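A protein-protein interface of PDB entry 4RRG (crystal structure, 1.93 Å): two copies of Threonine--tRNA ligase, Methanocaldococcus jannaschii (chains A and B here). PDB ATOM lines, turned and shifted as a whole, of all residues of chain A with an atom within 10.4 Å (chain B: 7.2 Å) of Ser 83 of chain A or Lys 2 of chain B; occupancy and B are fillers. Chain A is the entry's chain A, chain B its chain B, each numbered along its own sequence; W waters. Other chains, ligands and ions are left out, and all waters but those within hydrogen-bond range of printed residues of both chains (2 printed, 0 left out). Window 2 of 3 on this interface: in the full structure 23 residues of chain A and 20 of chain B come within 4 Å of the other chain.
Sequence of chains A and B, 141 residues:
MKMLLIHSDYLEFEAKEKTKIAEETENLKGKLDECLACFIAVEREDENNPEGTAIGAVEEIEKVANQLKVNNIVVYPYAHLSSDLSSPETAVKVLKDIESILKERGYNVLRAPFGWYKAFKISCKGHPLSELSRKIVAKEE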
ATOM      1  N   MET A   1     -37.909  25.381  -7.994  1.00  0.00           N
ATOM      2  CA  MET A   1     -38.094  24.968  -9.427  1.00  0.00           C
ATOM      3  C   MET A   1     -36.999  25.533 -10.337  1.00  0.00           C
ATOM      4  O   MET A   1     -36.565  26.664 -10.155  1.00  0.00           O
ATOM      5  CB  MET A   1     -39.459  25.436  -9.935  1.00  0.00           C
ATOM      6  CG  MET A   1     -39.668  25.236 -11.438  1.00  0.00           C
ATOM      7  SD  MET A   1     -41.279  25.774 -12.001  1.00  0.00           S
ATOM      8  CE  MET A   1     -42.299  24.399 -11.516  1.00  0.00           C
ATOM      9  N   LYS A   2     -36.572  24.743 -11.321  1.00  0.00           N
ATOM     10  CA  LYS A   2     -35.678  25.241 -12.363  1.00  0.00           C
ATOM     11  C   LYS A   2     -36.371  25.132 -13.709  1.00  0.00           C
ATOM     12  O   LYS A   2     -36.987  24.107 -14.031  1.00  0.00           O
ATOM     13  CB  LYS A   2     -34.331  24.486 -12.368  1.00  0.00           C
ATOM     14  CG  LYS A   2     -33.307  24.976 -13.407  1.00  0.00           C
ATOM     15  CD  LYS A   2     -32.540  26.222 -12.941  1.00  0.00           C
ATOM     16  CE  LYS A   2     -31.950  26.988 -14.111  1.00  0.00           C
ATOM     17  NZ  LYS A   2     -30.554  26.555 -14.460  1.00  0.00           N
ATOM     18  N   ILE A  40     -39.108  22.171 -17.666  1.00  0.00           N
ATOM     19  CA  ILE A  40     -39.302  22.357 -16.229  1.00  0.00           C
ATOM     20  C   ILE A  40     -38.896  21.143 -15.372  1.00  0.00           C
ATOM     21  O   ILE A  40     -39.304  20.021 -15.640  1.00  0.00           O
ATOM     22  CB  ILE A  40     -40.774  22.746 -15.926  1.00  0.00           C
ATOM     23  CG1 ILE A  40     -41.141  24.062 -16.640  1.00  0.00           C
ATOM     24  CG2 ILE A  40     -40.993  22.889 -14.422  1.00  0.00           C
ATOM     25  CD1 ILE A  40     -42.642  24.362 -16.675  1.00  0.00           C
ATOM     26  N   ALA A  41     -38.081  21.402 -14.356  1.00  0.00           N
ATOM     27  CA  ALA A  41     -37.787  20.427 -13.304  1.00  0.00           C
ATOM     28  C   ALA A  41     -38.423  20.930 -12.022  1.00  0.00           C
ATOM     29  O   ALA A  41     -38.051  21.996 -11.520  1.00  0.00           O
ATOM     30  CB  ALA A  41     -36.278  20.258 -13.117  1.00  0.00           C
ATOM     31  N   VAL A  42     -39.396  20.176 -11.522  1.00  0.00           N
ATOM     32  CA  VAL A  42     -40.037  20.469 -10.242  1.00  0.00           C
ATOM     33  C   VAL A  42     -39.130  19.895  -9.153  1.00  0.00           C
ATOM     34  O   VAL A  42     -38.765  18.721  -9.199  1.00  0.00           O
ATOM     35  CB  VAL A  42     -41.444  19.859 -10.161  1.00  0.00           C
ATOM     36  CG1 VAL A  42     -42.168  20.325  -8.893  1.00  0.00           C
ATOM     37  CG2 VAL A  42     -42.252  20.227 -11.406  1.00  0.00           C
ATOM     38  N   GLU A  43     -38.763  20.740  -8.197  1.00  0.00           N
ATOM     39  CA  GLU A  43     -37.676  20.442  -7.264  1.00  0.00           C
ATOM     40  C   GLU A  43     -38.184  20.088  -5.874  1.00  0.00           C
ATOM     41  O   GLU A  43     -39.330  20.366  -5.547  1.00  0.00           O
ATOM     42  CB  GLU A  43     -36.719  21.630  -7.190  1.00  0.00           C
ATOM     43  CG  GLU A  43     -35.954  21.871  -8.483  1.00  0.00           C
ATOM     44  CD  GLU A  43     -34.897  22.949  -8.360  1.00  0.00           C
ATOM     45  OE1 GLU A  43     -35.262  24.118  -8.158  1.00  0.00           O
ATOM     46  OE2 GLU A  43     -33.697  22.631  -8.479  1.00  0.00           O
ATOM     47  N   ARG A  44     -37.324  19.478  -5.058  1.00  0.00           N
ATOM     48  CA  ARG A  44     -37.713  19.052  -3.706  1.00  0.00           C
ATOM     49  C   ARG A  44     -38.239  20.235  -2.894  1.00  0.00           C
ATOM     50  O   ARG A  44     -39.262  20.112  -2.220  1.00  0.00           O
ATOM     51  CB  ARG A  44     -36.544  18.370  -2.986  1.00  0.00           C
ATOM     52  CG  ARG A  44     -36.893  17.778  -1.620  1.00  0.00           C
ATOM     53  CD  ARG A  44     -35.807  16.832  -1.096  1.00  0.00           C
ATOM     54  NE  ARG A  44     -34.463  17.414  -1.102  1.00  0.00           N
ATOM     55  CZ  ARG A  44     -33.938  18.124  -0.104  1.00  0.00           C
ATOM     56  NH1 ARG A  44     -34.644  18.362   0.995  1.00  0.00           N
ATOM     57  NH2 ARG A  44     -32.700  18.605  -0.205  1.00  0.00           N
ATOM     58  N   GLU A  45     -37.560  21.379  -2.987  1.00  0.00           N
ATOM     59  CA  GLU A  45     -38.000  22.607  -2.315  1.00  0.00           C
ATOM     60  C   GLU A  45     -39.413  23.049  -2.720  1.00  0.00           C
ATOM     61  O   GLU A  45     -40.111  23.706  -1.939  1.00  0.00           O
ATOM     62  CB  GLU A  45     -36.983  23.740  -2.515  1.00  0.00           C
ATOM     63  CG  GLU A  45     -35.830  23.698  -1.509  1.00  0.00           C
ATOM     64  CD  GLU A  45     -34.680  24.656  -1.827  1.00  0.00           C
ATOM     65  OE1 GLU A  45     -34.799  25.478  -2.769  1.00  0.00           O
ATOM     66  OE2 GLU A  45     -33.643  24.582  -1.126  1.00  0.00           O
ATOM     67  N   TYR A  78     -38.808  18.251 -17.677  1.00  0.00           N
ATOM     68  CA  TYR A  78     -37.388  18.017 -17.947  1.00  0.00           C
ATOM     69  C   TYR A  78     -36.579  17.887 -16.671  1.00  0.00           C
ATOM     70  O   TYR A  78     -35.990  18.852 -16.201  1.00  0.00           O
ATOM     71  CB  TYR A  78     -36.809  19.075 -18.895  1.00  0.00           C
ATOM     72  CG  TYR A  78     -35.854  18.470 -19.882  1.00  0.00           C
ATOM     73  CD1 TYR A  78     -36.325  17.695 -20.936  1.00  0.00           C
ATOM     74  CD2 TYR A  78     -34.480  18.645 -19.754  1.00  0.00           C
ATOM     75  CE1 TYR A  78     -35.461  17.115 -21.839  1.00  0.00           C
ATOM     76  CE2 TYR A  78     -33.595  18.059 -20.665  1.00  0.00           C
ATOM     77  CZ  TYR A  78     -34.098  17.298 -21.703  1.00  0.00           C
ATOM     78  OH  TYR A  78     -33.249  16.712 -22.619  1.00  0.00           O
ATOM     79  N   ALA A  79     -36.562  16.669 -16.132  1.00  0.00           N
ATOM     80  CA  ALA A  79     -35.939  16.374 -14.842  1.00  0.00           C
ATOM     81  C   ALA A  79     -34.453  16.720 -14.765  1.00  0.00           C
ATOM     82  O   ALA A  79     -33.965  17.144 -13.708  1.00  0.00           O
ATOM     83  CB  ALA A  79     -36.184  14.912 -14.447  1.00  0.00           C
ATOM     84  N   HIS A  80     -33.755  16.582 -15.895  1.00  0.00           N
ATOM     85  CA  HIS A  80     -32.316  16.845 -15.974  1.00  0.00           C
ATOM     86  C   HIS A  80     -31.862  18.257 -15.604  1.00  0.00           C
ATOM     87  O   HIS A  80     -30.664  18.486 -15.411  1.00  0.00           O
ATOM     88  CB  HIS A  80     -31.786  16.473 -17.363  1.00  0.00           C
ATOM     89  CG  HIS A  80     -31.804  15.007 -17.631  1.00  0.00           C
ATOM     90  ND1 HIS A  80     -31.972  14.479 -18.891  1.00  0.00           N
ATOM     91  CD2 HIS A  80     -31.707  13.949 -16.791  1.00  0.00           C
ATOM     92  CE1 HIS A  80     -31.946  13.160 -18.819  1.00  0.00           C
ATOM     93  NE2 HIS A  80     -31.786  12.815 -17.557  1.00  0.00           N
ATOM     94  N   LEU A  81     -32.797  19.201 -15.482  1.00  0.00           N
ATOM     95  CA  LEU A  81     -32.428  20.563 -15.083  1.00  0.00           C
ATOM     96  C   LEU A  81     -32.127  20.710 -13.590  1.00  0.00           C
ATOM     97  O   LEU A  81     -31.621  21.742 -13.159  1.00  0.00           O
ATOM     98  CB  LEU A  81     -33.478  21.584 -15.518  1.00  0.00           C
ATOM     99  CG  LEU A  81     -33.688  21.709 -17.022  1.00  0.00           C
ATOM    100  CD1 LEU A  81     -34.919  22.561 -17.301  1.00  0.00           C
ATOM    101  CD2 LEU A  81     -32.453  22.283 -17.731  1.00  0.00           C
ATOM    102  N   SER A  82     -32.430  19.679 -12.807  1.00  0.00           N
ATOM    103  CA  SER A  82     -32.143  19.707 -11.372  1.00  0.00           C
ATOM    104  C   SER A  82     -31.653  18.357 -10.858  1.00  0.00           C
ATOM    105  O   SER A  82     -32.016  17.315 -11.388  1.00  0.00           O
ATOM    106  CB  SER A  82     -33.385  20.155 -10.603  1.00  0.00           C
ATOM    107  OG  SER A  82     -33.162  20.172  -9.204  1.00  0.00           O
ATOM    108  N   SER A  83     -30.824  18.399  -9.820  1.00  0.00           N
ATOM    109  CA  SER A  83     -30.343  17.194  -9.161  1.00  0.00           C
ATOM    110  C   SER A  83     -31.093  16.890  -7.864  1.00  0.00           C
ATOM    111  O   SER A  83     -30.806  15.889  -7.205  1.00  0.00           O
ATOM    112  CB  SER A  83     -28.851  17.325  -8.865  1.00  0.00           C
ATOM    113  OG  SER A  83     -28.139  17.489 -10.073  1.00  0.00           O
ATOM    114  N   ASP A  84     -32.023  17.760  -7.483  1.00  0.00           N
ATOM    115  CA  ASP A  84     -32.795  17.568  -6.260  1.00  0.00           C
ATOM    116  C   ASP A  84     -34.274  17.704  -6.590  1.00  0.00           C
ATOM    117  O   ASP A  84     -34.880  18.761  -6.403  1.00  0.00           O
ATOM    118  CB  ASP A  84     -32.365  18.563  -5.177  1.00  0.00           C
ATOM    119  CG  ASP A  84     -32.930  18.222  -3.791  1.00  0.00           C
ATOM    120  OD1 ASP A  84     -33.422  17.095  -3.576  1.00  0.00           O
ATOM    121  OD2 ASP A  84     -32.875  19.095  -2.907  1.00  0.00           O
ATOM    122  N   LEU A  85     -34.840  16.612  -7.088  1.00  0.00           N
ATOM    123  CA  LEU A  85     -36.160  16.637  -7.704  1.00  0.00           C
ATOM    124  C   LEU A  85     -37.287  16.400  -6.717  1.00  0.00           C
ATOM    125  O   LEU A  85     -37.093  15.784  -5.669  1.00  0.00           O
ATOM    126  CB  LEU A  85     -36.234  15.587  -8.814  1.00  0.00           C
ATOM    127  CG  LEU A  85     -35.343  15.800 -10.039  1.00  0.00           C
ATOM    128  CD1 LEU A  85     -35.354  14.525 -10.886  1.00  0.00           C
ATOM    129  CD2 LEU A  85     -35.802  17.002 -10.843  1.00  0.00           C
ATOM    130  N   SER A  86     -38.471  16.883  -7.075  1.00  0.00           N
ATOM    131  CA  SER A  86     -39.681  16.581  -6.328  1.00  0.00           C
ATOM    132  C   SER A  86     -40.131  15.148  -6.598  1.00  0.00           C
ATOM    133  O   SER A  86     -39.582  14.459  -7.466  1.00  0.00           O
ATOM    134  CB  SER A  86     -40.804  17.536  -6.725  1.00  0.00           C
ATOM    135  OG  SER A  86     -41.508  17.055  -7.862  1.00  0.00           O
ATOM    136  N   LYS A 135     -34.738  30.296 -11.910  1.00  0.00           N
ATOM    137  CA  LYS A 135     -35.002  29.596 -10.675  1.00  0.00           C
ATOM    138  C   LYS A 135     -36.293  30.172 -10.105  1.00  0.00           C
ATOM    139  O   LYS A 135     -36.461  31.394 -10.034  1.00  0.00           O
ATOM    140  CB  LYS A 135     -33.850  29.783  -9.694  1.00  0.00           C
ATOM    141  CG  LYS A 135     -34.018  29.008  -8.400  1.00  0.00           C
ATOM    142  CD  LYS A 135     -33.500  27.583  -8.532  1.00  0.00           C
ATOM    143  CE  LYS A 135     -33.808  26.798  -7.273  1.00  0.00           C
ATOM    144  NZ  LYS A 135     -33.084  25.504  -7.167  1.00  0.00           N
ATOM    145  N   MET B   1     -18.625  20.651 -13.101  1.00  0.00           N
ATOM    146  CA  MET B   1     -19.222  20.735 -14.471  1.00  0.00           C
ATOM    147  C   MET B   1     -20.552  19.991 -14.546  1.00  0.00           C
ATOM    148  O   MET B   1     -20.705  18.922 -13.941  1.00  0.00           O
ATOM    149  CB  MET B   1     -18.247  20.160 -15.510  1.00  0.00           C
ATOM    150  CG  MET B   1     -18.821  20.077 -16.905  1.00  0.00           C
ATOM    151  SD  MET B   1     -17.617  19.486 -18.088  1.00  0.00           S
ATOM    152  CE  MET B   1     -16.664  20.972 -18.337  1.00  0.00           C
ATOM    153  N   LYS B   2     -21.504  20.555 -15.290  1.00  0.00           N
ATOM    154  CA  LYS B   2     -22.758  19.848 -15.618  1.00  0.00           C
ATOM    155  C   LYS B   2     -22.868  19.680 -17.119  1.00  0.00           C
ATOM    156  O   LYS B   2     -22.668  20.634 -17.867  1.00  0.00           O
ATOM    157  CB  LYS B   2     -23.982  20.609 -15.100  1.00  0.00           C
ATOM    158  CG  LYS B   2     -24.020  20.806 -13.586  1.00  0.00           C
ATOM    159  CD  LYS B   2     -24.881  19.756 -12.869  1.00  0.00           C
ATOM    160  CE  LYS B   2     -24.333  18.334 -12.981  1.00  0.00           C
ATOM    161  NZ  LYS B   2     -24.890  17.417 -11.930  1.00  0.00           N
ATOM    162  N   MET B   3     -23.175  18.468 -17.565  1.00  0.00           N
ATOM    163  CA  MET B   3     -23.350  18.211 -19.000  1.00  0.00           C
ATOM    164  C   MET B   3     -24.686  17.531 -19.245  1.00  0.00           C
ATOM    165  O   MET B   3     -25.118  16.704 -18.448  1.00  0.00           O
ATOM    166  CB  MET B   3     -22.253  17.283 -19.535  1.00  0.00           C
ATOM    167  CG  MET B   3     -20.822  17.759 -19.361  1.00  0.00           C
ATOM    168  SD  MET B   3     -19.638  16.594 -20.088  1.00  0.00           S
ATOM    169  CE  MET B   3     -20.578  16.004 -21.496  1.00  0.00           C
ATOM    170  N   LEU B   4     -25.328  17.886 -20.344  1.00  0.00           N
ATOM    171  CA  LEU B   4     -26.464  17.128 -20.838  1.00  0.00           C
ATOM    172  C   LEU B   4     -26.076  16.571 -22.201  1.00  0.00           C
ATOM    173  O   LEU B   4     -25.697  17.329 -23.100  1.00  0.00           O
ATOM    174  CB  LEU B   4     -27.718  18.004 -20.923  1.00  0.00           C
ATOM    175  CG  LEU B   4     -28.946  17.459 -21.675  1.00  0.00           C
ATOM    176  CD1 LEU B   4     -29.517  16.212 -21.031  1.00  0.00           C
ATOM    177  CD2 LEU B   4     -30.007  18.540 -21.750  1.00  0.00           C
ATOM    178  N   PHE B  39     -24.239  19.488 -24.300  1.00  0.00           N
ATOM    179  CA  PHE B  39     -24.470  20.816 -23.729  1.00  0.00           C
ATOM    180  C   PHE B  39     -23.740  20.933 -22.405  1.00  0.00           C
ATOM    181  O   PHE B  39     -23.980  20.152 -21.495  1.00  0.00           O
ATOM    182  CB  PHE B  39     -25.976  21.045 -23.602  1.00  0.00           C
ATOM    183  CG  PHE B  39     -26.686  21.017 -24.921  1.00  0.00           C
ATOM    184  CD1 PHE B  39     -26.915  22.201 -25.628  1.00  0.00           C
ATOM    185  CD2 PHE B  39     -27.107  19.808 -25.473  1.00  0.00           C
ATOM    186  CE1 PHE B  39     -27.558  22.175 -26.864  1.00  0.00           C
ATOM    187  CE2 PHE B  39     -27.732  19.763 -26.700  1.00  0.00           C
ATOM    188  CZ  PHE B  39     -27.981  20.944 -27.399  1.00  0.00           C
ATOM    189  N   ILE B  40     -22.809  21.883 -22.311  1.00  0.00           N
ATOM    190  CA  ILE B  40     -21.885  21.903 -21.185  1.00  0.00           C
ATOM    191  C   ILE B  40     -21.870  23.238 -20.427  1.00  0.00           C
ATOM    192  O   ILE B  40     -21.702  24.300 -21.032  1.00  0.00           O
ATOM    193  CB  ILE B  40     -20.446  21.527 -21.637  1.00  0.00           C
ATOM    194  CG1 ILE B  40     -20.426  20.145 -22.304  1.00  0.00           C
ATOM    195  CG2 ILE B  40     -19.484  21.539 -20.442  1.00  0.00           C
ATOM    196  CD1 ILE B  40     -19.142  19.861 -23.086  1.00  0.00           C
ATOM    197  N   ALA B  41     -22.080  23.166 -19.112  1.00  0.00           N
ATOM    198  CA  ALA B  41     -21.909  24.313 -18.223  1.00  0.00           C
ATOM    199  C   ALA B  41     -20.652  24.093 -17.379  1.00  0.00           C
ATOM    200  O   ALA B  41     -20.576  23.131 -16.605  1.00  0.00           O
ATOM    201  CB  ALA B  41     -23.128  24.485 -17.324  1.00  0.00           C
ATOM    202  N   VAL B  42     -19.664  24.965 -17.545  1.00  0.00           N
ATOM    203  CA  VAL B  42     -18.425  24.879 -16.771  1.00  0.00           C
ATOM    204  C   VAL B  42     -18.686  25.610 -15.456  1.00  0.00           C
ATOM    205  O   VAL B  42     -19.195  26.725 -15.461  1.00  0.00           O
ATOM    206  CB  VAL B  42     -17.222  25.484 -17.534  1.00  0.00           C
ATOM    207  CG1 VAL B  42     -15.935  25.305 -16.749  1.00  0.00           C
ATOM    208  CG2 VAL B  42     -17.064  24.823 -18.904  1.00  0.00           C
ATOM    209  N   GLU B  43     -18.368  24.969 -14.335  1.00  0.00           N
ATOM    210  CA  GLU B  43     -18.782  25.493 -13.032  1.00  0.00           C
ATOM    211  C   GLU B  43     -17.649  26.057 -12.192  1.00  0.00           C
ATOM    212  O   GLU B  43     -16.479  25.850 -12.484  1.00  0.00           O
ATOM    213  CB  GLU B  43     -19.522  24.423 -12.239  1.00  0.00           C
ATOM    214  CG  GLU B  43     -20.756  23.900 -12.942  1.00  0.00           C
ATOM    215  CD  GLU B  43     -21.469  22.862 -12.127  1.00  0.00           C
ATOM    216  OE1 GLU B  43     -20.891  21.777 -11.913  1.00  0.00           O
ATOM    217  OE2 GLU B  43     -22.608  23.137 -11.706  1.00  0.00           O
ATOM    218  N   ASP B  46     -14.840  23.945 -11.108  1.00  0.00           N
ATOM    219  CA  ASP B  46     -13.942  23.539 -12.191  1.00  0.00           C
ATOM    220  C   ASP B  46     -12.717  24.460 -12.347  1.00  0.00           C
ATOM    221  O   ASP B  46     -11.723  24.081 -12.971  1.00  0.00           O
ATOM    222  CB  ASP B  46     -14.701  23.449 -13.520  1.00  0.00           C
ATOM    223  CG  ASP B  46     -15.941  22.564 -13.441  1.00  0.00           C
ATOM    224  OD1 ASP B  46     -15.986  21.638 -12.603  1.00  0.00           O
ATOM    225  OD2 ASP B  46     -16.875  22.795 -14.243  1.00  0.00           O
ATOM    226  N   TYR B  78     -23.287  25.723 -22.762  1.00  0.00           N
ATOM    227  CA  TYR B  78     -24.664  25.896 -22.285  1.00  0.00           C
ATOM    228  C   TYR B  78     -24.718  26.252 -20.804  1.00  0.00           C
ATOM    229  O   TYR B  78     -24.983  25.399 -19.939  1.00  0.00           O
ATOM    230  CB  TYR B  78     -25.503  24.643 -22.576  1.00  0.00           C
ATOM    231  CG  TYR B  78     -26.919  24.977 -22.984  1.00  0.00           C
ATOM    232  CD1 TYR B  78     -27.174  25.731 -24.132  1.00  0.00           C
ATOM    233  CD2 TYR B  78     -27.999  24.547 -22.225  1.00  0.00           C
ATOM    234  CE1 TYR B  78     -28.474  26.055 -24.517  1.00  0.00           C
ATOM    235  CE2 TYR B  78     -29.307  24.862 -22.601  1.00  0.00           C
ATOM    236  CZ  TYR B  78     -29.535  25.619 -23.742  1.00  0.00           C
ATOM    237  OH  TYR B  78     -30.827  25.933 -24.109  1.00  0.00           O
ATOM    238  N   LEU B  81     -27.404  25.150 -17.764  1.00  0.00           N
ATOM    239  CA  LEU B  81     -27.464  23.919 -16.999  1.00  0.00           C
ATOM    240  C   LEU B  81     -27.029  24.083 -15.550  1.00  0.00           C
ATOM    241  O   LEU B  81     -27.345  23.240 -14.719  1.00  0.00           O
ATOM    242  CB  LEU B  81     -26.638  22.820 -17.678  1.00  0.00           C
ATOM    243  CG  LEU B  81     -27.133  22.398 -19.063  1.00  0.00           C
ATOM    244  CD1 LEU B  81     -26.171  21.393 -19.665  1.00  0.00           C
ATOM    245  CD2 LEU B  81     -28.534  21.816 -19.004  1.00  0.00           C
ATOM    246  N   SER B  82     -26.303  25.157 -15.248  1.00  0.00           N
ATOM    247  CA  SER B  82     -25.761  25.329 -13.906  1.00  0.00           C
ATOM    248  C   SER B  82     -25.989  26.713 -13.337  1.00  0.00           C
ATOM    249  O   SER B  82     -25.859  27.711 -14.041  1.00  0.00           O
ATOM    250  CB  SER B  82     -24.263  25.020 -13.883  1.00  0.00           C
ATOM    251  OG  SER B  82     -23.733  25.208 -12.578  1.00  0.00           O
ATOM    252  N   SER B  83     -26.291  26.753 -12.044  1.00  0.00           N
ATOM    253  CA  SER B  83     -26.489  28.013 -11.326  1.00  0.00           C
ATOM    254  C   SER B  83     -25.206  28.484 -10.637  1.00  0.00           C
ATOM    255  O   SER B  83     -25.220  29.509  -9.944  1.00  0.00           O
ATOM    256  CB  SER B  83     -27.607  27.871 -10.280  1.00  0.00           C
ATOM    257  OG  SER B  83     -28.718  27.139 -10.777  1.00  0.00           O
ATOM    258  N   SER B 133     -27.821  13.125 -18.211  1.00  0.00           N
ATOM    259  CA  SER B 133     -27.100  14.205 -17.548  1.00  0.00           C
ATOM    260  C   SER B 133     -25.989  13.646 -16.672  1.00  0.00           C
ATOM    261  O   SER B 133     -26.131  12.576 -16.074  1.00  0.00           O
ATOM    262  CB  SER B 133     -28.056  15.125 -16.781  1.00  0.00           C
ATOM    263  OG  SER B 133     -28.777  14.423 -15.794  1.00  0.00           O
ATOM    264  N   ARG B 134     -24.871  14.364 -16.635  1.00  0.00           N
ATOM    265  CA  ARG B 134     -23.700  13.947 -15.872  1.00  0.00           C
ATOM    266  C   ARG B 134     -23.090  15.113 -15.098  1.00  0.00           C
ATOM    267  O   ARG B 134     -22.984  16.223 -15.611  1.00  0.00           O
ATOM    268  CB  ARG B 134     -22.633  13.339 -16.791  1.00  0.00           C
ATOM    269  CG  ARG B 134     -23.075  12.087 -17.561  1.00  0.00           C
ATOM    270  CD  ARG B 134     -23.224  10.898 -16.634  1.00  0.00           C
ATOM    271  NE  ARG B 134     -23.538   9.673 -17.369  1.00  0.00           N
ATOM    272  CZ  ARG B 134     -24.759   9.168 -17.507  1.00  0.00           C
ATOM    273  NH1 ARG B 134     -25.802   9.774 -16.961  1.00  0.00           N
ATOM    274  NH2 ARG B 134     -24.932   8.044 -18.189  1.00  0.00           N
ATOM    275  N   LYS B 135     -22.709  14.832 -13.859  1.00  0.00           N
ATOM    276  CA  LYS B 135     -21.852  15.707 -13.061  1.00  0.00           C
ATOM    277  C   LYS B 135     -20.411  15.261 -13.265  1.00  0.00           C
ATOM    278  O   LYS B 135     -20.113  14.074 -13.174  1.00  0.00           O
ATOM    279  CB  LYS B 135     -22.217  15.598 -11.571  1.00  0.00           C
ATOM    280  CG  LYS B 135     -21.422  16.507 -10.639  1.00  0.00           C
ATOM    281  CD  LYS B 135     -22.085  17.869 -10.489  1.00  0.00           C
ATOM    282  CE  LYS B 135     -21.103  18.957 -10.076  1.00  0.00           C
ATOM    283  NZ  LYS B 135     -21.800  20.274  -9.964  1.00  0.00           N
ATOM    284  N   ILE B 136     -19.528  16.215 -13.551  1.00  0.00           N
ATOM    285  CA  ILE B 136     -18.097  15.949 -13.676  1.00  0.00           C
ATOM    286  C   ILE B 136     -17.346  16.723 -12.588  1.00  0.00           C
ATOM    287  O   ILE B 136     -17.580  17.919 -12.399  1.00  0.00           O
ATOM    288  CB  ILE B 136     -17.555  16.387 -15.065  1.00  0.00           C
ATOM    289  CG1 ILE B 136     -18.440  15.854 -16.208  1.00  0.00           C
ATOM    290  CG2 ILE B 136     -16.078  16.004 -15.219  1.00  0.00           C
ATOM    291  CD1 ILE B 136     -18.538  14.333 -16.296  1.00  0.00           C
HETATM  292  O   HOH W   1     -29.131  28.830 -14.120  1.00  0.00           O
HETATM  293  O   HOH W   2     -29.139  10.687 -16.833  1.00  0.00           O
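O of Lys 2 of chain B lies within hydrogen-bond range of N of Ala 41 of chain B (2.9 Å). The backbone NH (N) of Phe 39 of chain B sits at hydrogen-bond distance from the backbone carbonyl oxygen (O) of Leu 4 of chain B, at 2.9 Å. The backbone carbonyl oxygen (O) of Ile 40 of chain A is in hydrogen-bond range of the backbone NH (N) of Tyr 78 of chain A (2.7 Å).
Among the printed residues, merely in contact across the chains: Tyr 78 of chain A with Leu 4 of chain B (3.8 Å), His 80 of chain A with Leu 4 of chain B (3.7 Å), His 80 of chain A with Ser 133 of chain B (3.1 Å) and Ser 83 of chain A with Lys 2 of chain B (3.7 Å).
Of the printed residues of chain B, Tyr 78 of chain A touches Leu 4. Of the printed residues of chain B, His 80 of chain A touches Leu 4 and Ser 133. Of chain B, only Lys 2 comes within 4 Å of Ser 83 of chain A. No residue of chain A comes within 4 Å of Met 1 of chain B. Of chain A, only Ser 83 (3.7 Å) comes within 4 Å of Lys 2 of chain B. No residue of chain A comes within 4 Å of Met 3 of chain B. Of the printed residues of chain A, Leu 4 of chain B touches Tyr 78 and His 80. No residue of chain A comes within 4 Å of Ile 40 of chain B. No residue of chain A comes within 4 Å of Leu 81 of chain B. No residue of chain A comes within 4 Å of Lys 135 of chain B. The nearest residue of chain A that does not touch Lys 2 of chain B is His 80 of chain A (6.4 Å).
Hydrophobic or aromatic side chains of chain A within 4 Å of the printed part of chain B: Tyr 78 and His 80. Of the 18 printed residues of chain B, 3 touch a printed residue of chain A.
Ser 83 of chain A touches Lys 2 of chain B, but with the chains exchanged Lys 2 of chain A does not touch Ser 83 of chain B (4.2 Å). Of the 4 pairs that touch across the chains among the printed residues, none has its exchanged pair printed and touching as well.
Water W1 lies within hydrogen-bond range of NZ of Lys 2 of chain A (2.7 Å) and O of Ser 82 of chain B (3.5 Å). Water W2 lies within hydrogen-bond range of N of Ser 133 of chain B, NH1 of Arg 134 of chain B and NE2 of His 80 of chain A.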
